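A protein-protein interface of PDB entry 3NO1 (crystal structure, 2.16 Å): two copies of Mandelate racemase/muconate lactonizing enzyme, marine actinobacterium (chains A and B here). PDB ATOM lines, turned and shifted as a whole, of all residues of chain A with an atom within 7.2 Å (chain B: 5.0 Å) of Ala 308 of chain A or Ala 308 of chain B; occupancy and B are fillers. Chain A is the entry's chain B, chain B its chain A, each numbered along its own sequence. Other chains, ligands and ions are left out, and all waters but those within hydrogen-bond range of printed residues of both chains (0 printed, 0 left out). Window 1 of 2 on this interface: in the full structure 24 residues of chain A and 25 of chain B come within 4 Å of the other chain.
Hydrophobic or aromatic side chains of chain B that line the printed part of chain A: Ala 308 and Ile 309. Hydrophobic or aromatic side chains of chain A that line the printed part of chain B: Ala 308 and Ile 309. Among the printed residues, 8 pairs touch across the chains. Among the printed residues, no Asp or Glu carboxylate lies within 4 Å of a Lys or Arg side-chain nitrogen of the other chain.
The backbone carbonyl oxygen (O) of Ile 309 of chain A is in hydrogen-bond range of the side-chain hydroxyl (OG) of Ser 312 of chain A (2.6 Å). The backbone carbonyl oxygen (O) of Ala 308 of chain A sits at hydrogen-bond distance from the side-chain hydroxyl (OG1) of Thr 311 of chain A (2.7 Å). OG1 of Thr 311 of chain B is in hydrogen-bond range of O of Ala 308 of chain B, at 2.7 Å. The backbone carbonyl oxygen of Ile 309 of chain B is in hydrogen-bond range of the side-chain hydroxyl of Ser 312 of chain B (2.8 Å).
Of the printed residues of chain B, Arg 305 of chain A touches Ala 308 (3.8 Å) and Thr 311 (3.6 Å). Of the printed residues of chain B, Ile 309 of chain A touches Ile 309 (3.8 Å) and Ser 312 (3.6 Å). Of chain A, only Arg 305 and Ala 308 come within 4 Å of Ala 308 of chain B. Printed residues of chain A within 4 Å of Ser 312 of chain B: Ile 309. The nearest residue of chain B that does not touch Ala 308 of chain A is Ile 309 of chain B (4.3 Å). The nearest residue of chain A that does not touch Ala 308 of chain B is Ile 309 of chain A (4.4 Å). The nearest printed residue of chain B that does not touch Ser 312 of chain A is Arg 305 of chain B (6.2 Å).
Among the printed residues, pairs that only touch across the chains: Arg 305 of chain A with Ala 308 of chain B (3.8 Å), Arg 305 of chain A with Thr 311 of chain B (3.6 Å), Ala 308 of chain A with Arg 305 of chain B (3.8 Å), Ala 308 of chain A with Ala 308 of chain B (3.5 Å), Ile 309 of chain A with Ile 309 of chain B (3.8 Å), Ile 309 of chain A with Ser 312 of chain B (3.6 Å), Thr 311 of chain A with Arg 305 of chain B (3.5 Å) and Ser 312 of chain A with Ile 309 of chain B (3.6 Å).
Arg 305 of chain A touches Ala 308 of chain B, and with the chains exchanged Ala 308 of chain A touches Arg 305 of chain B. Ala 308 of chain B touches its own counterpart, Ala 308 of chain A. Ile 309 of chain B touches its own counterpart, Ile 309 of chain A. Ile 309 of chain A touches Ser 312 of chain B, and with the chains exchanged Ser 312 of chain A touches Ile 309 of chain B. 10 positions are printed for both chains.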
ATOM      1  N   ALA A 275      29.430 -25.901  -0.761  1.00  0.00           N
ATOM      2  CA  ALA A 275      28.230 -25.378  -0.118  1.00  0.00           C
ATOM      3  C   ALA A 275      27.000 -25.976  -0.795  1.00  0.00           C
ATOM      4  O   ALA A 275      25.952 -26.145  -0.166  1.00  0.00           O
ATOM      5  CB  ALA A 275      28.199 -23.862  -0.221  1.00  0.00           C
ATOM      6  N   MET A 282      20.722 -30.380   3.586  1.00  0.00           N
ATOM      7  CA  MET A 282      19.655 -29.599   4.211  1.00  0.00           C
ATOM      8  C   MET A 282      18.333 -29.697   3.469  1.00  0.00           C
ATOM      9  O   MET A 282      17.275 -29.845   4.082  1.00  0.00           O
ATOM     10  CB  MET A 282      20.086 -28.137   4.315  1.00  0.00           C
ATOM     11  CG  MET A 282      21.215 -27.920   5.313  1.00  0.00           C
ATOM     12  SD  MET A 282      21.907 -26.123   5.231  1.00  0.00           S
ATOM     13  CE  MET A 282      23.795 -26.490   5.326  1.00  0.00           C
ATOM     14  N   THR A 301      35.763 -18.695   3.287  1.00  0.00           N
ATOM     15  CA  THR A 301      34.819 -18.133   2.333  1.00  0.00           C
ATOM     16  C   THR A 301      33.741 -19.145   1.954  1.00  0.00           C
ATOM     17  O   THR A 301      32.554 -18.810   1.942  1.00  0.00           O
ATOM     18  CB  THR A 301      35.550 -17.600   1.080  1.00  0.00           C
ATOM     19  OG1 THR A 301      36.335 -16.461   1.458  1.00  0.00           O
ATOM     20  CG2 THR A 301      34.556 -17.182  -0.011  1.00  0.00           C
ATOM     21  N   ALA A 302      34.144 -20.386   1.683  1.00  0.00           N
ATOM     22  CA  ALA A 302      33.182 -21.432   1.327  1.00  0.00           C
ATOM     23  C   ALA A 302      32.320 -21.768   2.534  1.00  0.00           C
ATOM     24  O   ALA A 302      31.096 -21.873   2.432  1.00  0.00           O
ATOM     25  CB  ALA A 302      33.919 -22.689   0.849  1.00  0.00           C
ATOM     26  N   TRP A 303      32.966 -21.922   3.683  1.00  0.00           N
ATOM     27  CA  TRP A 303      32.272 -22.268   4.917  1.00  0.00           C
ATOM     28  C   TRP A 303      31.233 -21.231   5.314  1.00  0.00           C
ATOM     29  O   TRP A 303      30.125 -21.583   5.719  1.00  0.00           O
ATOM     30  CB  TRP A 303      33.274 -22.432   6.062  1.00  0.00           C
ATOM     31  CG  TRP A 303      32.690 -23.080   7.282  1.00  0.00           C
ATOM     32  CD1 TRP A 303      32.683 -24.411   7.577  1.00  0.00           C
ATOM     33  CD2 TRP A 303      32.043 -22.423   8.379  1.00  0.00           C
ATOM     34  NE1 TRP A 303      32.079 -24.628   8.789  1.00  0.00           N
ATOM     35  CE2 TRP A 303      31.676 -23.426   9.308  1.00  0.00           C
ATOM     36  CE3 TRP A 303      31.737 -21.086   8.670  1.00  0.00           C
ATOM     37  CZ2 TRP A 303      31.019 -23.136  10.511  1.00  0.00           C
ATOM     38  CZ3 TRP A 303      31.083 -20.795   9.866  1.00  0.00           C
ATOM     39  CH2 TRP A 303      30.733 -21.819  10.773  1.00  0.00           C
ATOM     40  N   LEU A 304      31.596 -19.955   5.206  1.00  0.00           N
ATOM     41  CA  LEU A 304      30.682 -18.875   5.563  1.00  0.00           C
ATOM     42  C   LEU A 304      29.463 -18.847   4.635  1.00  0.00           C
ATOM     43  O   LEU A 304      28.398 -18.375   5.016  1.00  0.00           O
ATOM     44  CB  LEU A 304      31.429 -17.530   5.562  1.00  0.00           C
ATOM     45  CG  LEU A 304      32.458 -17.470   6.707  1.00  0.00           C
ATOM     46  CD1 LEU A 304      33.377 -16.252   6.561  1.00  0.00           C
ATOM     47  CD2 LEU A 304      31.711 -17.464   8.050  1.00  0.00           C
ATOM     48  N   ARG A 305      29.618 -19.359   3.418  1.00  0.00           N
ATOM     49  CA  ARG A 305      28.494 -19.432   2.489  1.00  0.00           C
ATOM     50  C   ARG A 305      27.572 -20.528   3.015  1.00  0.00           C
ATOM     51  O   ARG A 305      26.362 -20.350   3.088  1.00  0.00           O
ATOM     52  CB  ARG A 305      28.967 -19.786   1.071  1.00  0.00           C
ATOM     53  CG  ARG A 305      29.706 -18.667   0.381  1.00  0.00           C
ATOM     54  CD  ARG A 305      30.105 -19.053  -1.023  1.00  0.00           C
ATOM     55  NE  ARG A 305      30.864 -17.991  -1.669  1.00  0.00           N
ATOM     56  CZ  ARG A 305      31.441 -18.105  -2.860  1.00  0.00           C
ATOM     57  NH1 ARG A 305      31.348 -19.246  -3.538  1.00  0.00           N
ATOM     58  NH2 ARG A 305      32.105 -17.077  -3.377  1.00  0.00           N
ATOM     59  N   THR A 306      28.155 -21.666   3.379  1.00  0.00           N
ATOM     60  CA  THR A 306      27.389 -22.774   3.930  1.00  0.00           C
ATOM     61  C   THR A 306      26.678 -22.305   5.207  1.00  0.00           C
ATOM     62  O   THR A 306      25.520 -22.649   5.442  1.00  0.00           O
ATOM     63  CB  THR A 306      28.312 -23.983   4.248  1.00  0.00           C
ATOM     64  OG1 THR A 306      28.944 -24.417   3.041  1.00  0.00           O
ATOM     65  CG2 THR A 306      27.517 -25.157   4.837  1.00  0.00           C
ATOM     66  N   ALA A 307      27.364 -21.504   6.023  1.00  0.00           N
ATOM     67  CA  ALA A 307      26.758 -20.995   7.252  1.00  0.00           C
ATOM     68  C   ALA A 307      25.504 -20.191   6.920  1.00  0.00           C
ATOM     69  O   ALA A 307      24.470 -20.353   7.560  1.00  0.00           O
ATOM     70  CB  ALA A 307      27.749 -20.127   8.014  1.00  0.00           C
ATOM     71  N   ALA A 308      25.595 -19.336   5.906  1.00  0.00           N
ATOM     72  CA  ALA A 308      24.459 -18.512   5.491  1.00  0.00           C
ATOM     73  C   ALA A 308      23.292 -19.384   5.023  1.00  0.00           C
ATOM     74  O   ALA A 308      22.136 -19.149   5.369  1.00  0.00           O
ATOM     75  CB  ALA A 308      24.887 -17.564   4.369  1.00  0.00           C
ATOM     76  N   ILE A 309      23.601 -20.392   4.220  1.00  0.00           N
ATOM     77  CA  ILE A 309      22.576 -21.296   3.724  1.00  0.00           C
ATOM     78  C   ILE A 309      21.894 -21.982   4.900  1.00  0.00           C
ATOM     79  O   ILE A 309      20.680 -22.157   4.897  1.00  0.00           O
ATOM     80  CB  ILE A 309      23.198 -22.362   2.790  1.00  0.00           C
ATOM     81  CG1 ILE A 309      23.862 -21.667   1.600  1.00  0.00           C
ATOM     82  CG2 ILE A 309      22.128 -23.328   2.305  1.00  0.00           C
ATOM     83  CD1 ILE A 309      24.602 -22.599   0.667  1.00  0.00           C
ATOM     84  N   ALA A 310      22.678 -22.352   5.910  1.00  0.00           N
ATOM     85  CA  ALA A 310      22.142 -23.022   7.096  1.00  0.00           C
ATOM     86  C   ALA A 310      21.130 -22.184   7.874  1.00  0.00           C
ATOM     87  O   ALA A 310      20.201 -22.737   8.464  1.00  0.00           O
ATOM     88  CB  ALA A 310      23.288 -23.454   8.030  1.00  0.00           C
ATOM     89  N   THR A 311      21.284 -20.859   7.887  1.00  0.00           N
ATOM     90  CA  THR A 311      20.320 -20.037   8.625  1.00  0.00           C
ATOM     91  C   THR A 311      18.959 -20.074   7.954  1.00  0.00           C
ATOM     92  O   THR A 311      17.929 -20.018   8.627  1.00  0.00           O
ATOM     93  CB  THR A 311      20.747 -18.543   8.755  1.00  0.00           C
ATOM     94  OG1 THR A 311      20.908 -17.961   7.456  1.00  0.00           O
ATOM     95  CG2 THR A 311      22.043 -18.421   9.541  1.00  0.00           C
ATOM     96  N   SER A 312      18.947 -20.178   6.625  1.00  0.00           N
ATOM     97  CA  SER A 312      17.686 -20.212   5.896  1.00  0.00           C
ATOM     98  C   SER A 312      16.949 -21.533   6.132  1.00  0.00           C
ATOM     99  O   SER A 312      15.749 -21.633   5.887  1.00  0.00           O
ATOM    100  CB  SER A 312      17.929 -19.994   4.387  1.00  0.00           C
ATOM    101  OG  SER A 312      18.557 -21.111   3.765  1.00  0.00           O
ATOM    102  N   TYR A 313      17.676 -22.533   6.624  1.00  0.00           N
ATOM    103  CA  TYR A 313      17.128 -23.866   6.916  1.00  0.00           C
ATOM    104  C   TYR A 313      16.999 -24.159   8.425  1.00  0.00           C
ATOM    105  O   TYR A 313      16.587 -25.255   8.814  1.00  0.00           O
ATOM    106  CB  TYR A 313      18.042 -24.941   6.310  1.00  0.00           C
ATOM    107  CG  TYR A 313      17.828 -25.248   4.834  1.00  0.00           C
ATOM    108  CD1 TYR A 313      16.822 -26.127   4.420  1.00  0.00           C
ATOM    109  CD2 TYR A 313      18.646 -24.685   3.859  1.00  0.00           C
ATOM    110  CE1 TYR A 313      16.643 -26.442   3.068  1.00  0.00           C
ATOM    111  CE2 TYR A 313      18.476 -24.992   2.501  1.00  0.00           C
ATOM    112  CZ  TYR A 313      17.468 -25.871   2.117  1.00  0.00           C
ATOM    113  OH  TYR A 313      17.289 -26.168   0.784  1.00  0.00           O
ATOM    114  N   MET A 317      25.487 -24.870  12.866  1.00  0.00           N
ATOM    115  CA  MET A 317      26.804 -25.105  12.293  1.00  0.00           C
ATOM    116  C   MET A 317      27.773 -25.733  13.289  1.00  0.00           C
ATOM    117  O   MET A 317      27.784 -25.412  14.477  1.00  0.00           O
ATOM    118  CB  MET A 317      27.417 -23.803  11.758  1.00  0.00           C
ATOM    119  CG  MET A 317      26.738 -23.229  10.518  1.00  0.00           C
ATOM    120  SD  MET A 317      26.714 -24.461   8.995  1.00  0.00           S
ATOM    121  CE  MET A 317      28.607 -24.661   8.694  1.00  0.00           C
ATOM    122  N   GLN A 333      29.168 -16.943  14.358  1.00  0.00           N
ATOM    123  CA  GLN A 333      27.777 -17.195  13.967  1.00  0.00           C
ATOM    124  C   GLN A 333      26.741 -17.412  15.067  1.00  0.00           C
ATOM    125  O   GLN A 333      27.019 -18.029  16.091  1.00  0.00           O
ATOM    126  CB  GLN A 333      27.744 -18.404  13.028  1.00  0.00           C
ATOM    127  CG  GLN A 333      28.659 -18.265  11.836  1.00  0.00           C
ATOM    128  CD  GLN A 333      28.204 -17.178  10.889  1.00  0.00           C
ATOM    129  OE1 GLN A 333      27.075 -17.202  10.407  1.00  0.00           O
ATOM    130  NE2 GLN A 333      29.083 -16.218  10.617  1.00  0.00           N
ATOM    131  N   HIS A 335      24.289 -19.377  14.996  1.00  0.00           N
ATOM    132  CA  HIS A 335      23.898 -20.778  15.046  1.00  0.00           C
ATOM    133  C   HIS A 335      25.093 -21.722  15.152  1.00  0.00           C
ATOM    134  O   HIS A 335      24.988 -22.913  14.847  1.00  0.00           O
ATOM    135  CB  HIS A 335      23.020 -21.124  13.829  1.00  0.00           C
ATOM    136  CG  HIS A 335      23.656 -20.825  12.504  1.00  0.00           C
ATOM    137  ND1 HIS A 335      24.461 -19.727  12.289  1.00  0.00           N
ATOM    138  CD2 HIS A 335      23.573 -21.469  11.314  1.00  0.00           C
ATOM    139  CE1 HIS A 335      24.849 -19.706  11.024  1.00  0.00           C
ATOM    140  NE2 HIS A 335      24.323 -20.753  10.412  1.00  0.00           N
ATOM    141  N   LEU B 304      22.969 -10.432   2.121  1.00  0.00           N
ATOM    142  CA  LEU B 304      24.211 -11.167   1.918  1.00  0.00           C
ATOM    143  C   LEU B 304      24.064 -12.672   2.159  1.00  0.00           C
ATOM    144  O   LEU B 304      24.814 -13.467   1.582  1.00  0.00           O
ATOM    145  CB  LEU B 304      25.321 -10.588   2.807  1.00  0.00           C
ATOM    146  CG  LEU B 304      25.739  -9.166   2.407  1.00  0.00           C
ATOM    147  CD1 LEU B 304      26.666  -8.576   3.460  1.00  0.00           C
ATOM    148  CD2 LEU B 304      26.423  -9.200   1.043  1.00  0.00           C
ATOM    149  N   ARG B 305      23.118 -13.065   3.013  1.00  0.00           N
ATOM    150  CA  ARG B 305      22.882 -14.481   3.270  1.00  0.00           C
ATOM    151  C   ARG B 305      22.228 -15.034   2.015  1.00  0.00           C
ATOM    152  O   ARG B 305      22.576 -16.111   1.540  1.00  0.00           O
ATOM    153  CB  ARG B 305      21.946 -14.684   4.465  1.00  0.00           C
ATOM    154  CG  ARG B 305      22.561 -14.354   5.810  1.00  0.00           C
ATOM    155  CD  ARG B 305      21.533 -14.537   6.919  1.00  0.00           C
ATOM    156  NE  ARG B 305      22.094 -14.243   8.230  1.00  0.00           N
ATOM    157  CZ  ARG B 305      21.425 -14.354   9.373  1.00  0.00           C
ATOM    158  NH1 ARG B 305      20.158 -14.752   9.374  1.00  0.00           N
ATOM    159  NH2 ARG B 305      22.030 -14.077  10.522  1.00  0.00           N
ATOM    160  N   THR B 306      21.268 -14.285   1.483  1.00  0.00           N
ATOM    161  CA  THR B 306      20.591 -14.688   0.264  1.00  0.00           C
ATOM    162  C   THR B 306      21.636 -14.831  -0.846  1.00  0.00           C
ATOM    163  O   THR B 306      21.612 -15.797  -1.612  1.00  0.00           O
ATOM    164  CB  THR B 306      19.524 -13.652  -0.133  1.00  0.00           C
ATOM    165  OG1 THR B 306      18.469 -13.670   0.835  1.00  0.00           O
ATOM    166  CG2 THR B 306      18.944 -13.967  -1.498  1.00  0.00           C
ATOM    167  N   ALA B 307      22.563 -13.879  -0.914  1.00  0.00           N
ATOM    168  CA  ALA B 307      23.626 -13.908  -1.914  1.00  0.00           C
ATOM    169  C   ALA B 307      24.418 -15.215  -1.843  1.00  0.00           C
ATOM    170  O   ALA B 307      24.679 -15.853  -2.866  1.00  0.00           O
ATOM    171  CB  ALA B 307      24.566 -12.720  -1.715  1.00  0.00           C
ATOM    172  N   ALA B 308      24.805 -15.601  -0.633  1.00  0.00           N
ATOM    173  CA  ALA B 308      25.567 -16.830  -0.421  1.00  0.00           C
ATOM    174  C   ALA B 308      24.780 -18.037  -0.928  1.00  0.00           C
ATOM    175  O   ALA B 308      25.321 -18.919  -1.588  1.00  0.00           O
ATOM    176  CB  ALA B 308      25.879 -16.997   1.059  1.00  0.00           C
ATOM    177  N   ILE B 309      23.499 -18.071  -0.605  1.00  0.00           N
ATOM    178  CA  ILE B 309      22.644 -19.160  -1.041  1.00  0.00           C
ATOM    179  C   ILE B 309      22.621 -19.192  -2.564  1.00  0.00           C
ATOM    180  O   ILE B 309      22.690 -20.267  -3.174  1.00  0.00           O
ATOM    181  CB  ILE B 309      21.228 -18.973  -0.509  1.00  0.00           C
ATOM    182  CG1 ILE B 309      21.270 -19.008   1.015  1.00  0.00           C
ATOM    183  CG2 ILE B 309      20.306 -20.082  -1.031  1.00  0.00           C
ATOM    184  CD1 ILE B 309      19.982 -18.594   1.666  1.00  0.00           C
ATOM    185  N   ALA B 310      22.542 -18.009  -3.172  1.00  0.00           N
ATOM    186  CA  ALA B 310      22.515 -17.894  -4.625  1.00  0.00           C
ATOM    187  C   ALA B 310      23.718 -18.564  -5.285  1.00  0.00           C
ATOM    188  O   ALA B 310      23.560 -19.245  -6.293  1.00  0.00           O
ATOM    189  CB  ALA B 310      22.427 -16.416  -5.052  1.00  0.00           C
ATOM    190  N   THR B 311      24.916 -18.380  -4.731  1.00  0.00           N
ATOM    191  CA  THR B 311      26.101 -19.007  -5.326  1.00  0.00           C
ATOM    192  C   THR B 311      25.992 -20.535  -5.381  1.00  0.00           C
ATOM    193  O   THR B 311      26.498 -21.155  -6.315  1.00  0.00           O
ATOM    194  CB  THR B 311      27.398 -18.692  -4.555  1.00  0.00           C
ATOM    195  OG1 THR B 311      27.366 -19.362  -3.287  1.00  0.00           O
ATOM    196  CG2 THR B 311      27.559 -17.177  -4.356  1.00  0.00           C
ATOM    197  N   SER B 312      25.350 -21.141  -4.385  1.00  0.00           N
ATOM    198  CA  SER B 312      25.227 -22.599  -4.360  1.00  0.00           C
ATOM    199  C   SER B 312      24.209 -23.094  -5.389  1.00  0.00           C
ATOM    200  O   SER B 312      24.210 -24.272  -5.754  1.00  0.00           O
ATOM    201  CB  SER B 312      24.850 -23.092  -2.956  1.00  0.00           C
ATOM    202  OG  SER B 312      23.462 -22.938  -2.702  1.00  0.00           O
ATOM    203  N   HIS B 335      28.666 -12.830  -8.400  1.00  0.00           N
ATOM    204  CA  HIS B 335      27.472 -13.097  -9.204  1.00  0.00           C
ATOM    205  C   HIS B 335      26.492 -11.930  -9.268  1.00  0.00           C
ATOM    206  O   HIS B 335      25.339 -12.094  -9.694  1.00  0.00           O
ATOM    207  CB  HIS B 335      26.759 -14.359  -8.682  1.00  0.00           C
ATOM    208  CG  HIS B 335      26.449 -14.332  -7.213  1.00  0.00           C
ATOM    209  ND1 HIS B 335      27.297 -13.771  -6.278  1.00  0.00           N
ATOM    210  CD2 HIS B 335      25.417 -14.860  -6.512  1.00  0.00           C
ATOM    211  CE1 HIS B 335      26.799 -13.954  -5.067  1.00  0.00           C
ATOM    212  NE2 HIS B 335      25.658 -14.614  -5.181  1.00  0.00           N
